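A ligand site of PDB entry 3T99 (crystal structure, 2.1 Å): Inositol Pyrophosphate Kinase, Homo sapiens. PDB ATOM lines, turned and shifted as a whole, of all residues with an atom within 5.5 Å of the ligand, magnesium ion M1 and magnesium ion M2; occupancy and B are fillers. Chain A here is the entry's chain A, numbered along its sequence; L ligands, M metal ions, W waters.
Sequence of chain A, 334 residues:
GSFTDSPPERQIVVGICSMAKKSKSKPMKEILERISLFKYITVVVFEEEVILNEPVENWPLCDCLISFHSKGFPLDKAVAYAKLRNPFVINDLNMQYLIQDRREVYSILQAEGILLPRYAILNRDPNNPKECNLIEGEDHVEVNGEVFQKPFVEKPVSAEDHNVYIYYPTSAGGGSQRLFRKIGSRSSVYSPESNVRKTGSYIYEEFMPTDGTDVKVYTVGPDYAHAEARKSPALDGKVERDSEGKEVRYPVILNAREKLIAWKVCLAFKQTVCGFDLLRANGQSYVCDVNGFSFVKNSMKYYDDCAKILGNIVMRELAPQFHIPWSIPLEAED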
ATOM      1  N   ARG A 102     -20.473   4.720 -20.822  1.00  0.00           N
ATOM      2  CA  ARG A 102     -20.763   5.813 -19.879  1.00  0.00           C
ATOM      3  C   ARG A 102     -19.814   5.821 -18.678  1.00  0.00           C
ATOM      4  O   ARG A 102     -19.559   6.887 -18.098  1.00  0.00           O
ATOM      5  CB  ARG A 102     -22.207   5.739 -19.373  1.00  0.00           C
ATOM      6  CG  ARG A 102     -23.256   6.030 -20.434  1.00  0.00           C
ATOM      7  CD  ARG A 102     -24.658   6.193 -19.853  1.00  0.00           C
ATOM      8  NE  ARG A 102     -25.663   5.975 -20.897  1.00  0.00           N
ATOM      9  CZ  ARG A 102     -26.087   6.901 -21.751  1.00  0.00           C
ATOM     10  NH1 ARG A 102     -25.615   8.130 -21.708  1.00  0.00           N
ATOM     11  NH2 ARG A 102     -26.989   6.591 -22.672  1.00  0.00           N
ATOM     12  N   TYR A 106     -17.488   9.042 -17.688  1.00  0.00           N
ATOM     13  CA  TYR A 106     -17.523   9.633 -16.379  1.00  0.00           C
ATOM     14  C   TYR A 106     -16.154   9.603 -15.683  1.00  0.00           C
ATOM     15  O   TYR A 106     -15.814  10.512 -14.918  1.00  0.00           O
ATOM     16  CB  TYR A 106     -18.597   8.969 -15.525  1.00  0.00           C
ATOM     17  CG  TYR A 106     -19.947   9.662 -15.599  1.00  0.00           C
ATOM     18  CD1 TYR A 106     -20.414  10.209 -16.797  1.00  0.00           C
ATOM     19  CD2 TYR A 106     -20.751   9.783 -14.463  1.00  0.00           C
ATOM     20  CE1 TYR A 106     -21.640  10.855 -16.862  1.00  0.00           C
ATOM     21  CE2 TYR A 106     -21.985  10.441 -14.512  1.00  0.00           C
ATOM     22  CZ  TYR A 106     -22.420  10.949 -15.719  1.00  0.00           C
ATOM     23  OH  TYR A 106     -23.627  11.600 -15.774  1.00  0.00           O
ATOM     24  N   PRO A 117     -22.612  14.868 -11.986  1.00  0.00           N
ATOM     25  CA  PRO A 117     -23.387  14.340 -10.870  1.00  0.00           C
ATOM     26  C   PRO A 117     -22.646  13.280 -10.014  1.00  0.00           C
ATOM     27  O   PRO A 117     -21.867  12.453 -10.541  1.00  0.00           O
ATOM     28  CB  PRO A 117     -24.612  13.691 -11.546  1.00  0.00           C
ATOM     29  CG  PRO A 117     -24.702  14.320 -12.886  1.00  0.00           C
ATOM     30  CD  PRO A 117     -23.318  14.731 -13.284  1.00  0.00           C
ATOM     31  N   VAL A 153     -31.334   9.143 -11.024  1.00  0.00           N
ATOM     32  CA  VAL A 153     -31.284   8.854 -12.447  1.00  0.00           C
ATOM     33  C   VAL A 153     -30.557   7.535 -12.642  1.00  0.00           C
ATOM     34  O   VAL A 153     -29.563   7.273 -11.978  1.00  0.00           O
ATOM     35  CB  VAL A 153     -30.607   9.990 -13.214  1.00  0.00           C
ATOM     36  CG1 VAL A 153     -30.652   9.724 -14.713  1.00  0.00           C
ATOM     37  CG2 VAL A 153     -31.276  11.302 -12.886  1.00  0.00           C
ATOM     38  N   LYS A 155     -28.915   5.058 -15.560  1.00  0.00           N
ATOM     39  CA  LYS A 155     -28.441   5.077 -16.946  1.00  0.00           C
ATOM     40  C   LYS A 155     -27.808   3.746 -17.376  1.00  0.00           C
ATOM     41  O   LYS A 155     -26.968   3.203 -16.672  1.00  0.00           O
ATOM     42  CB  LYS A 155     -27.437   6.219 -17.159  1.00  0.00           C
ATOM     43  CG  LYS A 155     -27.994   7.610 -16.888  1.00  0.00           C
ATOM     44  CD  LYS A 155     -26.982   8.673 -17.234  1.00  0.00           C
ATOM     45  CE  LYS A 155     -27.515  10.044 -16.996  1.00  0.00           C
ATOM     46  NZ  LYS A 155     -26.518  11.098 -17.366  1.00  0.00           N
ATOM     47  N   ALA A 159     -23.373   3.798 -23.711  1.00  0.00           N
ATOM     48  CA  ALA A 159     -23.793   5.172 -23.957  1.00  0.00           C
ATOM     49  C   ALA A 159     -24.712   5.259 -25.165  1.00  0.00           C
ATOM     50  O   ALA A 159     -25.259   6.316 -25.444  1.00  0.00           O
ATOM     51  CB  ALA A 159     -22.594   6.079 -24.130  1.00  0.00           C
ATOM     52  N   ASP A 161     -27.295   3.153 -25.546  1.00  0.00           N
ATOM     53  CA  ASP A 161     -28.616   2.775 -25.043  1.00  0.00           C
ATOM     54  C   ASP A 161     -29.234   4.003 -24.341  1.00  0.00           C
ATOM     55  O   ASP A 161     -28.802   4.426 -23.249  1.00  0.00           O
ATOM     56  CB  ASP A 161     -28.477   1.554 -24.117  1.00  0.00           C
ATOM     57  CG  ASP A 161     -29.807   1.046 -23.537  1.00  0.00           C
ATOM     58  OD1 ASP A 161     -30.861   1.720 -23.667  1.00  0.00           O
ATOM     59  OD2 ASP A 161     -29.780  -0.012 -22.889  1.00  0.00           O
ATOM     60  N   HIS A 162     -30.249   4.587 -24.974  1.00  0.00           N
ATOM     61  CA  HIS A 162     -30.843   5.827 -24.468  1.00  0.00           C
ATOM     62  C   HIS A 162     -32.016   5.622 -23.492  1.00  0.00           C
ATOM     63  O   HIS A 162     -32.714   6.565 -23.134  1.00  0.00           O
ATOM     64  CB  HIS A 162     -31.172   6.737 -25.636  1.00  0.00           C
ATOM     65  CG  HIS A 162     -29.996   6.989 -26.525  1.00  0.00           C
ATOM     66  ND1 HIS A 162     -29.022   7.911 -26.204  1.00  0.00           N
ATOM     67  CD2 HIS A 162     -29.588   6.386 -27.667  1.00  0.00           C
ATOM     68  CE1 HIS A 162     -28.085   7.889 -27.139  1.00  0.00           C
ATOM     69  NE2 HIS A 162     -28.404   6.987 -28.046  1.00  0.00           N
ATOM     70  N   VAL A 164     -32.879   5.780 -20.439  1.00  0.00           N
ATOM     71  CA  VAL A 164     -32.528   6.365 -19.135  1.00  0.00           C
ATOM     72  C   VAL A 164     -33.792   6.558 -18.285  1.00  0.00           C
ATOM     73  O   VAL A 164     -34.722   7.243 -18.698  1.00  0.00           O
ATOM     74  CB  VAL A 164     -31.785   7.728 -19.331  1.00  0.00           C
ATOM     75  CG1 VAL A 164     -31.759   8.558 -18.057  1.00  0.00           C
ATOM     76  CG2 VAL A 164     -30.362   7.510 -19.828  1.00  0.00           C
ATOM     77  N   ILE A 166     -35.658   7.875 -14.720  1.00  0.00           N
ATOM     78  CA  ILE A 166     -35.609   8.750 -13.562  1.00  0.00           C
ATOM     79  C   ILE A 166     -36.763   8.316 -12.633  1.00  0.00           C
ATOM     80  O   ILE A 166     -37.907   8.213 -13.085  1.00  0.00           O
ATOM     81  CB  ILE A 166     -35.811  10.235 -13.962  1.00  0.00           C
ATOM     82  CG1 ILE A 166     -34.787  10.661 -15.021  1.00  0.00           C
ATOM     83  CG2 ILE A 166     -35.747  11.132 -12.730  1.00  0.00           C
ATOM     84  CD1 ILE A 166     -35.072  11.997 -15.639  1.00  0.00           C
ATOM     85  N   LEU A 179     -37.155   7.630 -20.403  1.00  0.00           N
ATOM     86  CA  LEU A 179     -36.598   8.305 -21.561  1.00  0.00           C
ATOM     87  C   LEU A 179     -36.174   7.251 -22.580  1.00  0.00           C
ATOM     88  O   LEU A 179     -35.844   6.119 -22.220  1.00  0.00           O
ATOM     89  CB  LEU A 179     -35.394   9.203 -21.158  1.00  0.00           C
ATOM     90  CG  LEU A 179     -35.737  10.532 -20.447  1.00  0.00           C
ATOM     91  CD1 LEU A 179     -36.469  10.320 -19.113  1.00  0.00           C
ATOM     92  CD2 LEU A 179     -34.512  11.425 -20.235  1.00  0.00           C
ATOM     93  N   GLU A 205     -27.279   7.842 -10.403  1.00  0.00           N
ATOM     94  CA  GLU A 205     -26.739   9.160 -10.133  1.00  0.00           C
ATOM     95  C   GLU A 205     -27.753  10.134  -9.591  1.00  0.00           C
ATOM     96  O   GLU A 205     -28.970   9.998  -9.807  1.00  0.00           O
ATOM     97  CB  GLU A 205     -25.981   9.718 -11.355  1.00  0.00           C
ATOM     98  CG  GLU A 205     -26.805  10.121 -12.538  1.00  0.00           C
ATOM     99  CD  GLU A 205     -25.946  10.541 -13.722  1.00  0.00           C
ATOM    100  OE1 GLU A 205     -25.044   9.776 -14.106  1.00  0.00           O
ATOM    101  OE2 GLU A 205     -26.172  11.639 -14.274  1.00  0.00           O
ATOM    102  N   GLU A 206     -27.231  11.113  -8.862  1.00  0.00           N
ATOM    103  CA  GLU A 206     -28.009  12.162  -8.229  1.00  0.00           C
ATOM    104  C   GLU A 206     -28.739  12.992  -9.261  1.00  0.00           C
ATOM    105  O   GLU A 206     -28.158  13.372 -10.275  1.00  0.00           O
ATOM    106  CB  GLU A 206     -27.057  13.085  -7.456  1.00  0.00           C
ATOM    107  CG  GLU A 206     -27.772  14.074  -6.582  1.00  0.00           C
ATOM    108  CD  GLU A 206     -27.112  15.419  -6.534  1.00  0.00           C
ATOM    109  OE1 GLU A 206     -25.870  15.459  -6.297  1.00  0.00           O
ATOM    110  OE2 GLU A 206     -27.842  16.423  -6.737  1.00  0.00           O
ATOM    111  N   PHE A 207     -30.008  13.284  -8.992  1.00  0.00           N
ATOM    112  CA  PHE A 207     -30.800  14.101  -9.891  1.00  0.00           C
ATOM    113  C   PHE A 207     -30.492  15.578  -9.700  1.00  0.00           C
ATOM    114  O   PHE A 207     -30.735  16.139  -8.641  1.00  0.00           O
ATOM    115  CB  PHE A 207     -32.309  13.837  -9.678  1.00  0.00           C
ATOM    116  CG  PHE A 207     -33.211  14.722 -10.513  1.00  0.00           C
ATOM    117  CD1 PHE A 207     -33.741  15.900  -9.986  1.00  0.00           C
ATOM    118  CD2 PHE A 207     -33.564  14.358 -11.809  1.00  0.00           C
ATOM    119  CE1 PHE A 207     -34.574  16.729 -10.755  1.00  0.00           C
ATOM    120  CE2 PHE A 207     -34.416  15.181 -12.589  1.00  0.00           C
ATOM    121  CZ  PHE A 207     -34.931  16.372 -12.047  1.00  0.00           C
ATOM    122  N   MET A 208     -29.987  16.223 -10.755  1.00  0.00           N
ATOM    123  CA  MET A 208     -29.699  17.664 -10.741  1.00  0.00           C
ATOM    124  C   MET A 208     -30.923  18.487 -11.059  1.00  0.00           C
ATOM    125  O   MET A 208     -31.444  18.440 -12.177  1.00  0.00           O
ATOM    126  CB  MET A 208     -28.575  18.014 -11.735  1.00  0.00           C
ATOM    127  CG  MET A 208     -27.301  17.225 -11.529  1.00  0.00           C
ATOM    128  SD  MET A 208     -26.780  17.047  -9.807  1.00  0.00           S
ATOM    129  CE  MET A 208     -26.480  18.752  -9.331  1.00  0.00           C
ATOM    130  N   PRO A 209     -31.413  19.256 -10.067  1.00  0.00           N
ATOM    131  CA  PRO A 209     -32.634  20.014 -10.304  1.00  0.00           C
ATOM    132  C   PRO A 209     -32.333  21.204 -11.199  1.00  0.00           C
ATOM    133  O   PRO A 209     -31.622  22.115 -10.774  1.00  0.00           O
ATOM    134  CB  PRO A 209     -33.036  20.465  -8.900  1.00  0.00           C
ATOM    135  CG  PRO A 209     -31.764  20.476  -8.120  1.00  0.00           C
ATOM    136  CD  PRO A 209     -30.882  19.434  -8.697  1.00  0.00           C
ATOM    137  N   THR A 210     -32.860  21.187 -12.411  1.00  0.00           N
ATOM    138  CA  THR A 210     -32.662  22.302 -13.348  1.00  0.00           C
ATOM    139  C   THR A 210     -33.979  23.023 -13.567  1.00  0.00           C
ATOM    140  O   THR A 210     -35.001  22.640 -12.993  1.00  0.00           O
ATOM    141  CB  THR A 210     -32.164  21.835 -14.737  1.00  0.00           C
ATOM    142  OG1 THR A 210     -33.259  21.298 -15.491  1.00  0.00           O
ATOM    143  CG2 THR A 210     -31.040  20.805 -14.616  1.00  0.00           C
ATOM    144  N   ASP A 214     -32.312  21.523 -20.953  1.00  0.00           N
ATOM    145  CA  ASP A 214     -30.981  20.946 -21.057  1.00  0.00           C
ATOM    146  C   ASP A 214     -30.165  21.908 -21.872  1.00  0.00           C
ATOM    147  O   ASP A 214     -30.632  22.404 -22.916  1.00  0.00           O
ATOM    148  CB  ASP A 214     -31.022  19.627 -21.816  1.00  0.00           C
ATOM    149  CG  ASP A 214     -31.549  18.474 -20.998  1.00  0.00           C
ATOM    150  OD1 ASP A 214     -31.552  18.530 -19.758  1.00  0.00           O
ATOM    151  OD2 ASP A 214     -31.929  17.463 -21.627  1.00  0.00           O
ATOM    152  N   LYS A 216     -27.345  22.208 -24.497  1.00  0.00           N
ATOM    153  CA  LYS A 216     -26.619  21.414 -25.474  1.00  0.00           C
ATOM    154  C   LYS A 216     -25.436  22.239 -25.976  1.00  0.00           C
ATOM    155  O   LYS A 216     -25.627  23.360 -26.435  1.00  0.00           O
ATOM    156  CB  LYS A 216     -27.533  21.020 -26.638  1.00  0.00           C
ATOM    157  CG  LYS A 216     -28.854  20.371 -26.218  1.00  0.00           C
ATOM    158  CD  LYS A 216     -28.659  18.900 -25.932  1.00  0.00           C
ATOM    159  CE  LYS A 216     -29.973  18.171 -25.745  1.00  0.00           C
ATOM    160  NZ  LYS A 216     -29.736  16.900 -24.984  1.00  0.00           N
ATOM    161  N   SER A 232     -36.372  19.619 -21.242  1.00  0.00           N
ATOM    162  CA  SER A 232     -35.885  18.366 -20.712  1.00  0.00           C
ATOM    163  C   SER A 232     -36.839  17.243 -21.110  1.00  0.00           C
ATOM    164  O   SER A 232     -38.037  17.326 -20.818  1.00  0.00           O
ATOM    165  CB  SER A 232     -35.738  18.428 -19.191  1.00  0.00           C
ATOM    166  OG  SER A 232     -35.466  17.119 -18.692  1.00  0.00           O
ATOM    167  N   PRO A 233     -36.324  16.185 -21.770  1.00  0.00           N
ATOM    168  CA  PRO A 233     -37.182  15.086 -22.235  1.00  0.00           C
ATOM    169  C   PRO A 233     -38.034  14.449 -21.135  1.00  0.00           C
ATOM    170  O   PRO A 233     -39.128  13.954 -21.421  1.00  0.00           O
ATOM    171  CB  PRO A 233     -36.171  14.071 -22.773  1.00  0.00           C
ATOM    172  CG  PRO A 233     -35.007  14.868 -23.164  1.00  0.00           C
ATOM    173  CD  PRO A 233     -34.927  15.975 -22.162  1.00  0.00           C
ATOM    174  N   ALA A 234     -37.556  14.491 -19.904  1.00  0.00           N
ATOM    175  CA  ALA A 234     -38.268  13.926 -18.768  1.00  0.00           C
ATOM    176  C   ALA A 234     -39.456  14.748 -18.291  1.00  0.00           C
ATOM    177  O   ALA A 234     -40.200  14.314 -17.401  1.00  0.00           O
ATOM    178  CB  ALA A 234     -37.313  13.714 -17.618  1.00  0.00           C
ATOM    179  N   ASP A 277     -23.775  17.456 -23.010  1.00  0.00           N
ATOM    180  CA  ASP A 277     -24.928  18.061 -22.335  1.00  0.00           C
ATOM    181  C   ASP A 277     -24.526  18.743 -21.018  1.00  0.00           C
ATOM    182  O   ASP A 277     -23.769  18.176 -20.259  1.00  0.00           O
ATOM    183  CB  ASP A 277     -26.008  17.014 -22.072  1.00  0.00           C
ATOM    184  CG  ASP A 277     -26.654  16.496 -23.366  1.00  0.00           C
ATOM    185  OD1 ASP A 277     -26.803  17.258 -24.335  1.00  0.00           O
ATOM    186  OD2 ASP A 277     -27.025  15.312 -23.413  1.00  0.00           O
ATOM    187  N   LEU A 279     -26.150  20.404 -17.346  1.00  0.00           N
ATOM    188  CA  LEU A 279     -27.263  20.667 -16.440  1.00  0.00           C
ATOM    189  C   LEU A 279     -26.912  21.864 -15.564  1.00  0.00           C
ATOM    190  O   LEU A 279     -26.032  21.762 -14.697  1.00  0.00           O
ATOM    191  CB  LEU A 279     -27.585  19.435 -15.583  1.00  0.00           C
ATOM    192  CG  LEU A 279     -27.830  18.150 -16.390  1.00  0.00           C
ATOM    193  CD1 LEU A 279     -27.834  16.951 -15.491  1.00  0.00           C
ATOM    194  CD2 LEU A 279     -29.126  18.235 -17.191  1.00  0.00           C
ATOM    195  N   CYS A 288     -23.509  15.751 -18.057  1.00  0.00           N
ATOM    196  CA  CYS A 288     -24.152  14.443 -17.785  1.00  0.00           C
ATOM    197  C   CYS A 288     -24.010  13.439 -18.945  1.00  0.00           C
ATOM    198  O   CYS A 288     -24.354  12.254 -18.810  1.00  0.00           O
ATOM    199  CB  CYS A 288     -25.625  14.625 -17.396  1.00  0.00           C
ATOM    200  SG  CYS A 288     -26.678  15.305 -18.716  1.00  0.00           S
ATOM    201  N   ASP A 289     -23.481  13.917 -20.064  1.00  0.00           N
ATOM    202  CA  ASP A 289     -23.470  13.159 -21.289  1.00  0.00           C
ATOM    203  C   ASP A 289     -22.422  13.755 -22.212  1.00  0.00           C
ATOM    204  O   ASP A 289     -22.381  14.965 -22.388  1.00  0.00           O
ATOM    205  CB  ASP A 289     -24.875  13.249 -21.922  1.00  0.00           C
ATOM    206  CG  ASP A 289     -25.053  12.351 -23.129  1.00  0.00           C
ATOM    207  OD1 ASP A 289     -24.379  11.296 -23.238  1.00  0.00           O
ATOM    208  OD2 ASP A 289     -25.897  12.691 -24.008  1.00  0.00           O
ATOM    209  N   VAL A 290     -21.557  12.920 -22.775  1.00  0.00           N
ATOM    210  CA  VAL A 290     -20.606  13.351 -23.801  1.00  0.00           C
ATOM    211  C   VAL A 290     -20.750  12.455 -25.023  1.00  0.00           C
ATOM    212  O   VAL A 290     -20.541  11.252 -24.908  1.00  0.00           O
ATOM    213  CB  VAL A 290     -19.125  13.337 -23.310  1.00  0.00           C
ATOM    214  CG1 VAL A 290     -18.202  13.732 -24.447  1.00  0.00           C
ATOM    215  CG2 VAL A 290     -18.937  14.312 -22.147  1.00  0.00           C
ATOM    216  N   ASN A 291     -21.076  13.046 -26.175  1.00  0.00           N
ATOM    217  CA  ASN A 291     -21.528  12.282 -27.357  1.00  0.00           C
ATOM    218  C   ASN A 291     -20.578  12.261 -28.555  1.00  0.00           C
ATOM    219  O   ASN A 291     -20.779  11.516 -29.519  1.00  0.00           O
ATOM    220  CB  ASN A 291     -22.923  12.776 -27.785  1.00  0.00           C
ATOM    221  CG  ASN A 291     -23.955  12.661 -26.657  1.00  0.00           C
ATOM    222  OD1 ASN A 291     -24.038  11.622 -26.019  1.00  0.00           O
ATOM    223  ND2 ASN A 291     -24.695  13.748 -26.384  1.00  0.00           N
HETATM  224  P1  LIG L   1     -28.315  10.208 -23.421  1.00  0.00           P
HETATM  225  O1  LIG L   1     -29.332   9.044 -23.884  1.00  0.00           O
HETATM  226  O2  LIG L   1     -26.894   9.661 -23.786  1.00  0.00           O
HETATM  227  O3  LIG L   1     -28.590  11.461 -24.163  1.00  0.00           O
HETATM  228  P2  LIG L   1     -28.161  11.595 -20.939  1.00  0.00           P
HETATM  229  O4  LIG L   1     -27.125  11.336 -19.906  1.00  0.00           O
HETATM  230  O5  LIG L   1     -28.092  12.777 -21.830  1.00  0.00           O
HETATM  231  O6  LIG L   1     -28.308  10.265 -21.820  1.00  0.00           O
HETATM  232  O7  LIG L   1     -29.613  11.667 -20.182  1.00  0.00           O
HETATM  233  C1  LIG L   1     -30.817  11.996 -20.891  1.00  0.00           C
HETATM  234  C2  LIG L   1     -31.562  13.201 -20.260  1.00  0.00           C
HETATM  235  O8  LIG L   1     -31.748  12.771 -18.878  1.00  0.00           O
HETATM  236  C3  LIG L   1     -30.659  14.421 -20.088  1.00  0.00           C
HETATM  237  O9  LIG L   1     -30.617  15.243 -21.240  1.00  0.00           O
HETATM  238  C4  LIG L   1     -31.362  15.140 -18.959  1.00  0.00           C
HETATM  239  O10 LIG L   1     -32.485  15.904 -19.424  1.00  0.00           O
HETATM  240  C5  LIG L   1     -31.786  13.989 -18.054  1.00  0.00           C
HETATM  241  N1  LIG L   1     -30.706  13.843 -17.023  1.00  0.00           N
HETATM  242  C6  LIG L   1     -29.481  13.034 -17.257  1.00  0.00           C
HETATM  243  N2  LIG L   1     -28.937  12.885 -15.920  1.00  0.00           N
HETATM  244  C7  LIG L   1     -29.566  13.767 -15.136  1.00  0.00           C
HETATM  245  C8  LIG L   1     -29.313  14.167 -13.823  1.00  0.00           C
HETATM  246  N3  LIG L   1     -28.305  13.632 -13.146  1.00  0.00           N
HETATM  247  N4  LIG L   1     -30.111  15.095 -13.272  1.00  0.00           N
HETATM  248  C9  LIG L   1     -31.140  15.625 -13.937  1.00  0.00           C
HETATM  249  N5  LIG L   1     -31.425  15.273 -15.182  1.00  0.00           N
HETATM  250  C10 LIG L   1     -30.649  14.359 -15.811  1.00  0.00           C
HETATM  251 MG    MG M   1     -27.916  13.376 -23.664  1.00  0.00          MG
HETATM  252 MG    MG M   2     -25.527  10.753 -24.919  1.00  0.00          MG
HETATM  253  O   HOH W   1     -29.721  14.423 -23.706  1.00  0.00           O
HETATM  254  O   HOH W   2     -33.314  17.134 -16.101  1.00  0.00           O
HETATM  255  O   HOH W   3     -27.662  13.718 -25.520  1.00  0.00           O
HETATM  256  O   HOH W   4     -31.895   9.158 -22.930  1.00  0.00           O
HETATM  257  O   HOH W   5     -24.273   9.702 -19.894  1.00  0.00           O
HETATM  258  O   HOH W   6     -24.636   9.096 -25.257  1.00  0.00           O
HETATM  259  O   HOH W   7     -26.558  10.866 -26.507  1.00  0.00           O
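Water W1 lies within hydrogen-bond range of O9 of the ligand (2.7 Å) and NZ of Lys 216 (2.8 Å).
Water W4 lies within hydrogen-bond range of O of His 162 (2.7 Å) and O1 of the ligand (2.7 Å).
Water W2 lies within hydrogen-bond range of N5 of the ligand and OG of Ser 232.
Water W5 lies within hydrogen-bond range of NH1 of Arg 102 (2.8 Å), O of Cys 288 (2.8 Å) and O4 of the ligand (3.3 Å).
The side-chain carboxylate (OD1) of Asp 289 lies close to the guanidinium group (NH1) of Arg 102, at 3.7 Å.
NZ of Lys 216 lies within salt-bridge range of OD1 of Asp 277.
NZ of Lys 155 is in hydrogen-bond range of O of Cys 288 (2.8 Å).
OE2 of Glu 205 lies within salt-bridge range of NZ of Lys 155.
O of Ala 159 is in hydrogen-bond range of NH2 of Arg 102, 3.3 Å away.
The guanidinium group (NH2) of Arg 102 lies within hydrogen-bond range of the backbone carbonyl oxygen (O) of Asp 161, 2.9 Å away.
The backbone carbonyl oxygen (O) of Cys 288 lies within hydrogen-bond range of the side-chain hydroxyl (OH) of Tyr 106, 3.2 Å away.
The side-chain carboxylate (OE1) of Glu 205 is in hydrogen-bond range of the side-chain hydroxyl (OH) of Tyr 106 (2.8 Å).
Magnesium ion M1 is bound by water W3 (1.9 Å), O5 of the ligand (1.9 Å), water W1 (2.1 Å), O3 of the ligand (2.1 Å), OD2 of Asp 277 (2.1 Å) and OD2 of Asp 289 (2.2 Å).
Magnesium ion M1 has six donor atoms within binding distance.
Magnesium ion M2 is bound by water W7 (1.9 Å), water W6 (1.9 Å), the side-chain amide oxygen (OD1) of Asn 291 (2.0 Å), an oxygen (O2) of the ligand (2.1 Å), the side-chain carboxylate (OD1) of Asp 289 (2.1 Å) and the side-chain carboxylate (OD2) of Asp 289 (2.2 Å).
Of the 28 residues printed, 2 come within 4 Å of magnesium ion M2.
A ring nitrogen (ND1) of His 162 sits at hydrogen-bond distance from an oxygen (O1) of the ligand, at 2.6 Å.
OD2 of Asp 214 lies within hydrogen-bond range of O9 of the ligand (2.6 Å).
The side-chain amino group (NZ) of Lys 155 lies within salt-bridge range of an oxygen (O4) of the ligand, at 2.6 Å.
N4 of the ligand is in hydrogen-bond range of N of Met 208 (2.8 Å).
An oxygen (O1) of the ligand is in salt-bridge range of the guanidinium group of Arg 102.
The backbone carbonyl oxygen (O) of Glu 206 sits at hydrogen-bond distance from a nitrogen (N3) of the ligand, at 2.9 Å.
The side-chain carboxylate (OE2) of Glu 205 is in hydrogen-bond range of a nitrogen (N3) of the ligand (3.1 Å).
O10 of the ligand lies within hydrogen-bond range of OG of Ser 232 (3.3 Å).
O4 of the ligand lies close to O of Cys 288 (3.1 Å).
Merely in contact with the ligand: Leu 179, Phe 207, Leu 279, Val 153, Pro 233, Pro 117 and Val 164.
Of the 28 residues printed, 18 come within 4 Å of the ligand.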
